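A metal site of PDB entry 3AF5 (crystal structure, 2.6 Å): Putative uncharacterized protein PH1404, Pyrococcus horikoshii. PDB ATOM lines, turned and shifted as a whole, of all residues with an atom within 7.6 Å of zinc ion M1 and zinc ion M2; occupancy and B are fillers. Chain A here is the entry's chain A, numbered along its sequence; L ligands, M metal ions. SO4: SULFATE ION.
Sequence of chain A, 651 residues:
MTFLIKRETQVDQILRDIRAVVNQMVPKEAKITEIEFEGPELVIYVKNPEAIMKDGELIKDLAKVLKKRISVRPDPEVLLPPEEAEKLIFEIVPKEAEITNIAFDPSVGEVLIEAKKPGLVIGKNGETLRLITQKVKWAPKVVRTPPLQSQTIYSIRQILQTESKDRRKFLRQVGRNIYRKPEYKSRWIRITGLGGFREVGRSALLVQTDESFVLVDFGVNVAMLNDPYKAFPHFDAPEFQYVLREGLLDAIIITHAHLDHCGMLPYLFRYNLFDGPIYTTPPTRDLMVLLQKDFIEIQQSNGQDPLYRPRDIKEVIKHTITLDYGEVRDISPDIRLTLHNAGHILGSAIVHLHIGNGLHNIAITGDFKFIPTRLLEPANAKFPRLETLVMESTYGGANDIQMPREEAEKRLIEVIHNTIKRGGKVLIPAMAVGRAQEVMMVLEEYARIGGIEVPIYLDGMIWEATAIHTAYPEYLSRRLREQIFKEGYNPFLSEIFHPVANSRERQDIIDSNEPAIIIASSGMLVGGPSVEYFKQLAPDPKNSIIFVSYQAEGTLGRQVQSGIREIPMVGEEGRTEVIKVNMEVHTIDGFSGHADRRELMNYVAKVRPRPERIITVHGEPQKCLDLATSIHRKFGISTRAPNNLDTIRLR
Zinc ion M1 is bound by a ring nitrogen (ND1) of His 258 (2.2 Å), a ring nitrogen (NE2) of His 256 (2.3 Å), a ring nitrogen (NE2) of His 344 (2.3 Å) and the side-chain carboxylate (OD1) of Asp 367 (2.6 Å).
Along chain A the residues within 4 Å of zinc ion M1 span positions 256 to 367. The nearest printed residue that does not touch zinc ion M1 is His 261 (4.3 Å).
Of the 25 residues printed, 4 come within 4 Å of zinc ion M2.
The backbone carbonyl oxygen (O) of His 618 lies within hydrogen-bond range of the backbone NH (N) of Thr 394, 3.0 Å away. The backbone carbonyl oxygen (O) of His 344 sits at hydrogen-bond distance from the guanidinium group (NH2) of Arg 435 (3.2 Å). OD2 of Asp 217 sits at hydrogen-bond distance from ND1 of His 261, at 2.7 Å. ND1 of His 344 is in hydrogen-bond range of O of Gly 593, 2.8 Å away. The side-chain hydroxyl (OG) of Ser 348 sits at hydrogen-bond distance from the backbone NH (N) of His 344. OG1 of Thr 255 lies within hydrogen-bond range of ND1 of His 256 (2.9 Å). NE2 of His 258 sits at hydrogen-bond distance from O of Val 433, at 3.0 Å. OD1 of Asp 260 sits close to NE2 of His 261 (3.2 Å).
Zinc ion M2 is bound by NE2 of His 261, NE2 of His 618, OD1 of Asp 367 and O3 of the ligand. Zinc ion M2 has four donor atoms within binding distance. Slightly farther from zinc ion M2 lies OD1 of Asp 260 (2.8 Å).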
ATOM      1  N   VAL A 200      20.141 -10.075   8.302  1.00  0.00           N
ATOM      2  CA  VAL A 200      20.574 -10.439   6.964  1.00  0.00           C
ATOM      3  C   VAL A 200      22.020  -9.976   6.903  1.00  0.00           C
ATOM      4  O   VAL A 200      22.306  -8.802   7.075  1.00  0.00           O
ATOM      5  CB  VAL A 200      19.736  -9.706   5.887  1.00  0.00           C
ATOM      6  CG1 VAL A 200      20.358  -9.921   4.515  1.00  0.00           C
ATOM      7  CG2 VAL A 200      18.309 -10.225   5.913  1.00  0.00           C
ATOM      8  N   GLY A 201      22.939 -10.909   6.672  1.00  0.00           N
ATOM      9  CA  GLY A 201      24.344 -10.540   6.602  1.00  0.00           C
ATOM     10  C   GLY A 201      25.214 -11.503   7.393  1.00  0.00           C
ATOM     11  O   GLY A 201      24.751 -12.108   8.379  1.00  0.00           O
ATOM     12  N   ARG A 202      26.457 -11.662   6.963  1.00  0.00           N
ATOM     13  CA  ARG A 202      27.431 -12.533   7.619  1.00  0.00           C
ATOM     14  C   ARG A 202      26.920 -13.896   8.063  1.00  0.00           C
ATOM     15  O   ARG A 202      27.159 -14.313   9.199  1.00  0.00           O
ATOM     16  CB  ARG A 202      28.035 -11.824   8.840  1.00  0.00           C
ATOM     17  CG  ARG A 202      27.010 -11.473   9.926  1.00  0.00           C
ATOM     18  CD  ARG A 202      27.659 -10.984  11.209  1.00  0.00           C
ATOM     19  NE  ARG A 202      26.664 -10.501  12.149  1.00  0.00           N
ATOM     20  CZ  ARG A 202      26.942  -9.846  13.271  1.00  0.00           C
ATOM     21  NH1 ARG A 202      28.206  -9.616  13.589  1.00  0.00           N
ATOM     22  NH2 ARG A 202      25.971  -9.410  14.062  1.00  0.00           N
ATOM     23  N   SER A 203      26.223 -14.605   7.171  1.00  0.00           N
ATOM     24  CA  SER A 203      25.733 -15.933   7.513  1.00  0.00           C
ATOM     25  C   SER A 203      26.886 -16.859   7.908  1.00  0.00           C
ATOM     26  O   SER A 203      27.874 -17.007   7.178  1.00  0.00           O
ATOM     27  CB  SER A 203      24.971 -16.550   6.332  1.00  0.00           C
ATOM     28  OG  SER A 203      23.683 -15.985   6.191  1.00  0.00           O
ATOM     29  N   ASP A 217      28.654 -21.827   5.498  1.00  0.00           N
ATOM     30  CA  ASP A 217      28.726 -20.415   5.119  1.00  0.00           C
ATOM     31  C   ASP A 217      29.616 -19.645   6.074  1.00  0.00           C
ATOM     32  O   ASP A 217      29.868 -20.080   7.209  1.00  0.00           O
ATOM     33  CB  ASP A 217      27.349 -19.758   5.037  1.00  0.00           C
ATOM     34  CG  ASP A 217      26.636 -20.052   3.721  1.00  0.00           C
ATOM     35  OD1 ASP A 217      27.271 -20.684   2.839  1.00  0.00           O
ATOM     36  OD2 ASP A 217      25.457 -19.666   3.552  1.00  0.00           O
ATOM     37  N   THR A 255      26.922 -22.296   0.585  1.00  0.00           N
ATOM     38  CA  THR A 255      25.660 -22.443  -0.130  1.00  0.00           C
ATOM     39  C   THR A 255      25.669 -21.757  -1.496  1.00  0.00           C
ATOM     40  O   THR A 255      25.163 -22.327  -2.473  1.00  0.00           O
ATOM     41  CB  THR A 255      24.484 -21.879   0.674  1.00  0.00           C
ATOM     42  OG1 THR A 255      24.659 -20.471   0.843  1.00  0.00           O
ATOM     43  CG2 THR A 255      24.391 -22.563   2.020  1.00  0.00           C
ATOM     44  N   HIS A 256      26.203 -20.541  -1.557  1.00  0.00           N
ATOM     45  CA  HIS A 256      26.310 -19.815  -2.823  1.00  0.00           C
ATOM     46  C   HIS A 256      27.331 -18.677  -2.793  1.00  0.00           C
ATOM     47  O   HIS A 256      27.822 -18.273  -1.739  1.00  0.00           O
ATOM     48  CB  HIS A 256      24.947 -19.299  -3.287  1.00  0.00           C
ATOM     49  CG  HIS A 256      24.333 -18.262  -2.401  1.00  0.00           C
ATOM     50  ND1 HIS A 256      23.873 -18.547  -1.126  1.00  0.00           N
ATOM     51  CD2 HIS A 256      23.986 -16.975  -2.641  1.00  0.00           C
ATOM     52  CE1 HIS A 256      23.278 -17.480  -0.631  1.00  0.00           C
ATOM     53  NE2 HIS A 256      23.329 -16.510  -1.533  1.00  0.00           N
ATOM     54  N   ALA A 257      27.646 -18.167  -3.975  1.00  0.00           N
ATOM     55  CA  ALA A 257      28.661 -17.144  -4.144  1.00  0.00           C
ATOM     56  C   ALA A 257      28.529 -15.761  -3.517  1.00  0.00           C
ATOM     57  O   ALA A 257      29.531 -15.054  -3.432  1.00  0.00           O
ATOM     58  CB  ALA A 257      28.958 -16.993  -5.613  1.00  0.00           C
ATOM     59  N   HIS A 258      27.352 -15.346  -3.065  1.00  0.00           N
ATOM     60  CA  HIS A 258      27.255 -14.007  -2.485  1.00  0.00           C
ATOM     61  C   HIS A 258      28.165 -13.695  -1.267  1.00  0.00           C
ATOM     62  O   HIS A 258      28.458 -14.572  -0.446  1.00  0.00           O
ATOM     63  CB  HIS A 258      25.787 -13.689  -2.180  1.00  0.00           C
ATOM     64  CG  HIS A 258      24.990 -13.400  -3.411  1.00  0.00           C
ATOM     65  ND1 HIS A 258      23.684 -13.822  -3.568  1.00  0.00           N
ATOM     66  CD2 HIS A 258      25.301 -12.716  -4.531  1.00  0.00           C
ATOM     67  CE1 HIS A 258      23.234 -13.405  -4.741  1.00  0.00           C
ATOM     68  NE2 HIS A 258      24.194 -12.738  -5.346  1.00  0.00           N
ATOM     69  N   LEU A 259      28.608 -12.447  -1.172  1.00  0.00           N
ATOM     70  CA  LEU A 259      29.524 -12.048  -0.104  1.00  0.00           C
ATOM     71  C   LEU A 259      29.021 -12.227   1.330  1.00  0.00           C
ATOM     72  O   LEU A 259      29.826 -12.413   2.236  1.00  0.00           O
ATOM     73  CB  LEU A 259      29.988 -10.605  -0.318  1.00  0.00           C
ATOM     74  CG  LEU A 259      30.941 -10.301  -1.482  1.00  0.00           C
ATOM     75  CD1 LEU A 259      31.236  -8.807  -1.506  1.00  0.00           C
ATOM     76  CD2 LEU A 259      32.244 -11.070  -1.348  1.00  0.00           C
ATOM     77  N   ASP A 260      27.717 -12.165   1.544  1.00  0.00           N
ATOM     78  CA  ASP A 260      27.245 -12.355   2.904  1.00  0.00           C
ATOM     79  C   ASP A 260      27.065 -13.831   3.241  1.00  0.00           C
ATOM     80  O   ASP A 260      26.436 -14.180   4.223  1.00  0.00           O
ATOM     81  CB  ASP A 260      25.947 -11.571   3.163  1.00  0.00           C
ATOM     82  CG  ASP A 260      24.759 -12.168   2.468  1.00  0.00           C
ATOM     83  OD1 ASP A 260      23.844 -12.634   3.178  1.00  0.00           O
ATOM     84  OD2 ASP A 260      24.746 -12.158   1.217  1.00  0.00           O
ATOM     85  N   HIS A 261      27.647 -14.686   2.408  1.00  0.00           N
ATOM     86  CA  HIS A 261      27.608 -16.123   2.645  1.00  0.00           C
ATOM     87  C   HIS A 261      28.992 -16.735   2.498  1.00  0.00           C
ATOM     88  O   HIS A 261      29.255 -17.808   3.030  1.00  0.00           O
ATOM     89  CB  HIS A 261      26.640 -16.806   1.680  1.00  0.00           C
ATOM     90  CG  HIS A 261      25.207 -16.506   1.973  1.00  0.00           C
ATOM     91  ND1 HIS A 261      24.441 -17.279   2.815  1.00  0.00           N
ATOM     92  CD2 HIS A 261      24.422 -15.477   1.589  1.00  0.00           C
ATOM     93  CE1 HIS A 261      23.238 -16.745   2.938  1.00  0.00           C
ATOM     94  NE2 HIS A 261      23.198 -15.650   2.207  1.00  0.00           N
ATOM     95  N   HIS A 344      18.515 -19.954  -6.547  1.00  0.00           N
ATOM     96  CA  HIS A 344      18.749 -18.567  -6.146  1.00  0.00           C
ATOM     97  C   HIS A 344      19.613 -17.814  -7.170  1.00  0.00           C
ATOM     98  O   HIS A 344      19.233 -16.742  -7.635  1.00  0.00           O
ATOM     99  CB  HIS A 344      19.417 -18.573  -4.781  1.00  0.00           C
ATOM    100  CG  HIS A 344      19.750 -17.213  -4.259  1.00  0.00           C
ATOM    101  ND1 HIS A 344      18.794 -16.237  -4.073  1.00  0.00           N
ATOM    102  CD2 HIS A 344      20.917 -16.685  -3.845  1.00  0.00           C
ATOM    103  CE1 HIS A 344      19.356 -15.163  -3.569  1.00  0.00           C
ATOM    104  NE2 HIS A 344      20.652 -15.409  -3.422  1.00  0.00           N
ATOM    105  N   ILE A 345      20.774 -18.373  -7.484  1.00  0.00           N
ATOM    106  CA  ILE A 345      21.681 -17.811  -8.488  1.00  0.00           C
ATOM    107  C   ILE A 345      22.487 -19.001  -8.991  1.00  0.00           C
ATOM    108  O   ILE A 345      22.457 -20.071  -8.380  1.00  0.00           O
ATOM    109  CB  ILE A 345      22.699 -16.763  -7.917  1.00  0.00           C
ATOM    110  CG1 ILE A 345      23.739 -17.478  -7.046  1.00  0.00           C
ATOM    111  CG2 ILE A 345      21.962 -15.638  -7.155  1.00  0.00           C
ATOM    112  CD1 ILE A 345      24.829 -16.561  -6.532  1.00  0.00           C
ATOM    113  N   SER A 348      23.793 -21.984  -6.787  1.00  0.00           N
ATOM    114  CA  SER A 348      23.301 -21.936  -5.404  1.00  0.00           C
ATOM    115  C   SER A 348      22.789 -23.295  -4.943  1.00  0.00           C
ATOM    116  O   SER A 348      22.025 -23.950  -5.672  1.00  0.00           O
ATOM    117  CB  SER A 348      22.211 -20.872  -5.248  1.00  0.00           C
ATOM    118  OG  SER A 348      21.051 -21.192  -5.987  1.00  0.00           O
ATOM    119  N   GLY A 366      20.160 -21.833   2.861  1.00  0.00           N
ATOM    120  CA  GLY A 366      20.942 -20.771   2.256  1.00  0.00           C
ATOM    121  C   GLY A 366      19.874 -19.863   1.677  1.00  0.00           C
ATOM    122  O   GLY A 366      18.786 -19.730   2.248  1.00  0.00           O
ATOM    123  N   ASP A 367      20.119 -19.204   0.554  1.00  0.00           N
ATOM    124  CA  ASP A 367      19.043 -18.402  -0.012  1.00  0.00           C
ATOM    125  C   ASP A 367      18.442 -19.293  -1.086  1.00  0.00           C
ATOM    126  O   ASP A 367      19.149 -20.067  -1.738  1.00  0.00           O
ATOM    127  CB  ASP A 367      19.591 -17.126  -0.625  1.00  0.00           C
ATOM    128  CG  ASP A 367      20.135 -16.175   0.415  1.00  0.00           C
ATOM    129  OD1 ASP A 367      20.862 -15.247   0.034  1.00  0.00           O
ATOM    130  OD2 ASP A 367      19.841 -16.366   1.604  1.00  0.00           O
ATOM    131  N   PHE A 368      17.120 -19.224  -1.247  1.00  0.00           N
ATOM    132  CA  PHE A 368      16.483 -20.058  -2.245  1.00  0.00           C
ATOM    133  C   PHE A 368      15.271 -19.405  -2.854  1.00  0.00           C
ATOM    134  O   PHE A 368      14.687 -18.463  -2.295  1.00  0.00           O
ATOM    135  CB  PHE A 368      16.092 -21.429  -1.648  1.00  0.00           C
ATOM    136  CG  PHE A 368      14.891 -21.388  -0.752  1.00  0.00           C
ATOM    137  CD1 PHE A 368      14.978 -20.923   0.543  1.00  0.00           C
ATOM    138  CD2 PHE A 368      13.654 -21.835  -1.222  1.00  0.00           C
ATOM    139  CE1 PHE A 368      13.857 -20.880   1.382  1.00  0.00           C
ATOM    140  CE2 PHE A 368      12.513 -21.799  -0.406  1.00  0.00           C
ATOM    141  CZ  PHE A 368      12.614 -21.325   0.900  1.00  0.00           C
ATOM    142  N   GLU A 392      15.801 -19.493   5.213  1.00  0.00           N
ATOM    143  CA  GLU A 392      15.895 -18.050   5.189  1.00  0.00           C
ATOM    144  C   GLU A 392      14.543 -17.364   5.380  1.00  0.00           C
ATOM    145  O   GLU A 392      13.484 -17.957   5.150  1.00  0.00           O
ATOM    146  CB  GLU A 392      16.504 -17.592   3.856  1.00  0.00           C
ATOM    147  CG  GLU A 392      15.619 -17.863   2.624  1.00  0.00           C
ATOM    148  CD  GLU A 392      15.729 -16.744   1.578  1.00  0.00           C
ATOM    149  OE1 GLU A 392      15.319 -15.601   1.878  1.00  0.00           O
ATOM    150  OE2 GLU A 392      16.245 -16.996   0.471  1.00  0.00           O
ATOM    151  N   THR A 394      14.266 -13.762   4.430  1.00  0.00           N
ATOM    152  CA  THR A 394      14.398 -12.438   3.829  1.00  0.00           C
ATOM    153  C   THR A 394      13.042 -11.767   3.627  1.00  0.00           C
ATOM    154  O   THR A 394      12.907 -10.576   3.865  1.00  0.00           O
ATOM    155  CB  THR A 394      15.136 -12.500   2.486  1.00  0.00           C
ATOM    156  OG1 THR A 394      16.340 -13.248   2.642  1.00  0.00           O
ATOM    157  CG2 THR A 394      15.494 -11.092   2.040  1.00  0.00           C
ATOM    158  N   VAL A 433      26.629 -10.889  -9.784  1.00  0.00           N
ATOM    159  CA  VAL A 433      25.975 -12.180  -9.994  1.00  0.00           C
ATOM    160  C   VAL A 433      24.607 -12.140  -9.333  1.00  0.00           C
ATOM    161  O   VAL A 433      24.470 -11.714  -8.178  1.00  0.00           O
ATOM    162  CB  VAL A 433      26.760 -13.320  -9.330  1.00  0.00           C
ATOM    163  CG1 VAL A 433      26.178 -14.645  -9.767  1.00  0.00           C
ATOM    164  CG2 VAL A 433      28.224 -13.227  -9.698  1.00  0.00           C
ATOM    165  N   ARG A 435      20.717 -10.703  -9.777  1.00  0.00           N
ATOM    166  CA  ARG A 435      19.724  -9.928 -10.495  1.00  0.00           C
ATOM    167  C   ARG A 435      20.239  -9.416 -11.843  1.00  0.00           C
ATOM    168  O   ARG A 435      19.464  -9.229 -12.772  1.00  0.00           O
ATOM    169  CB  ARG A 435      19.245  -8.717  -9.667  1.00  0.00           C
ATOM    170  CG  ARG A 435      18.430  -9.009  -8.395  1.00  0.00           C
ATOM    171  CD  ARG A 435      17.487 -10.200  -8.506  1.00  0.00           C
ATOM    172  NE  ARG A 435      18.196 -11.433  -8.179  1.00  0.00           N
ATOM    173  CZ  ARG A 435      17.985 -12.615  -8.744  1.00  0.00           C
ATOM    174  NH1 ARG A 435      17.046 -12.744  -9.678  1.00  0.00           N
ATOM    175  NH2 ARG A 435      18.719 -13.657  -8.376  1.00  0.00           N
ATOM    176  N   GLY A 593      15.561 -12.824  -6.135  1.00  0.00           N
ATOM    177  CA  GLY A 593      16.099 -14.170  -6.132  1.00  0.00           C
ATOM    178  C   GLY A 593      15.681 -14.871  -4.863  1.00  0.00           C
ATOM    179  O   GLY A 593      16.075 -16.004  -4.615  1.00  0.00           O
ATOM    180  N   HIS A 594      14.903 -14.184  -4.028  1.00  0.00           N
ATOM    181  CA  HIS A 594      14.430 -14.759  -2.759  1.00  0.00           C
ATOM    182  C   HIS A 594      12.980 -15.170  -2.840  1.00  0.00           C
ATOM    183  O   HIS A 594      12.168 -14.483  -3.456  1.00  0.00           O
ATOM    184  CB  HIS A 594      14.541 -13.740  -1.622  1.00  0.00           C
ATOM    185  CG  HIS A 594      15.933 -13.378  -1.253  1.00  0.00           C
ATOM    186  ND1 HIS A 594      16.787 -14.253  -0.600  1.00  0.00           N
ATOM    187  CD2 HIS A 594      16.638 -12.229  -1.436  1.00  0.00           C
ATOM    188  CE1 HIS A 594      17.940 -13.652  -0.392  1.00  0.00           C
ATOM    189  NE2 HIS A 594      17.876 -12.432  -0.892  1.00  0.00           N
ATOM    190  N   HIS A 618      18.319 -15.647   8.571  1.00  0.00           N
ATOM    191  CA  HIS A 618      18.566 -14.772   7.441  1.00  0.00           C
ATOM    192  C   HIS A 618      17.358 -13.909   7.064  1.00  0.00           C
ATOM    193  O   HIS A 618      16.738 -14.115   6.026  1.00  0.00           O
ATOM    194  CB  HIS A 618      19.007 -15.634   6.262  1.00  0.00           C
ATOM    195  CG  HIS A 618      19.558 -14.873   5.102  1.00  0.00           C
ATOM    196  ND1 HIS A 618      18.802 -13.977   4.370  1.00  0.00           N
ATOM    197  CD2 HIS A 618      20.775 -14.907   4.513  1.00  0.00           C
ATOM    198  CE1 HIS A 618      19.532 -13.510   3.370  1.00  0.00           C
ATOM    199  NE2 HIS A 618      20.733 -14.055   3.439  1.00  0.00           N
HETATM  200  S   SO4 L   1      21.256 -11.462   0.051  1.00  0.00           S
HETATM  201  O1  SO4 L   1      21.144  -9.997  -0.097  1.00  0.00           O
HETATM  202  O2  SO4 L   1      22.581 -11.886  -0.406  1.00  0.00           O
HETATM  203  O3  SO4 L   1      21.061 -11.827   1.459  1.00  0.00           O
HETATM  204  O4  SO4 L   1      20.226 -12.128  -0.784  1.00  0.00           O
HETATM  205 ZN    ZN M   1      22.285 -14.577  -2.021  1.00  0.00          ZN
HETATM  206 ZN    ZN M   2      21.960 -14.024   1.610  1.00  0.00          ZN
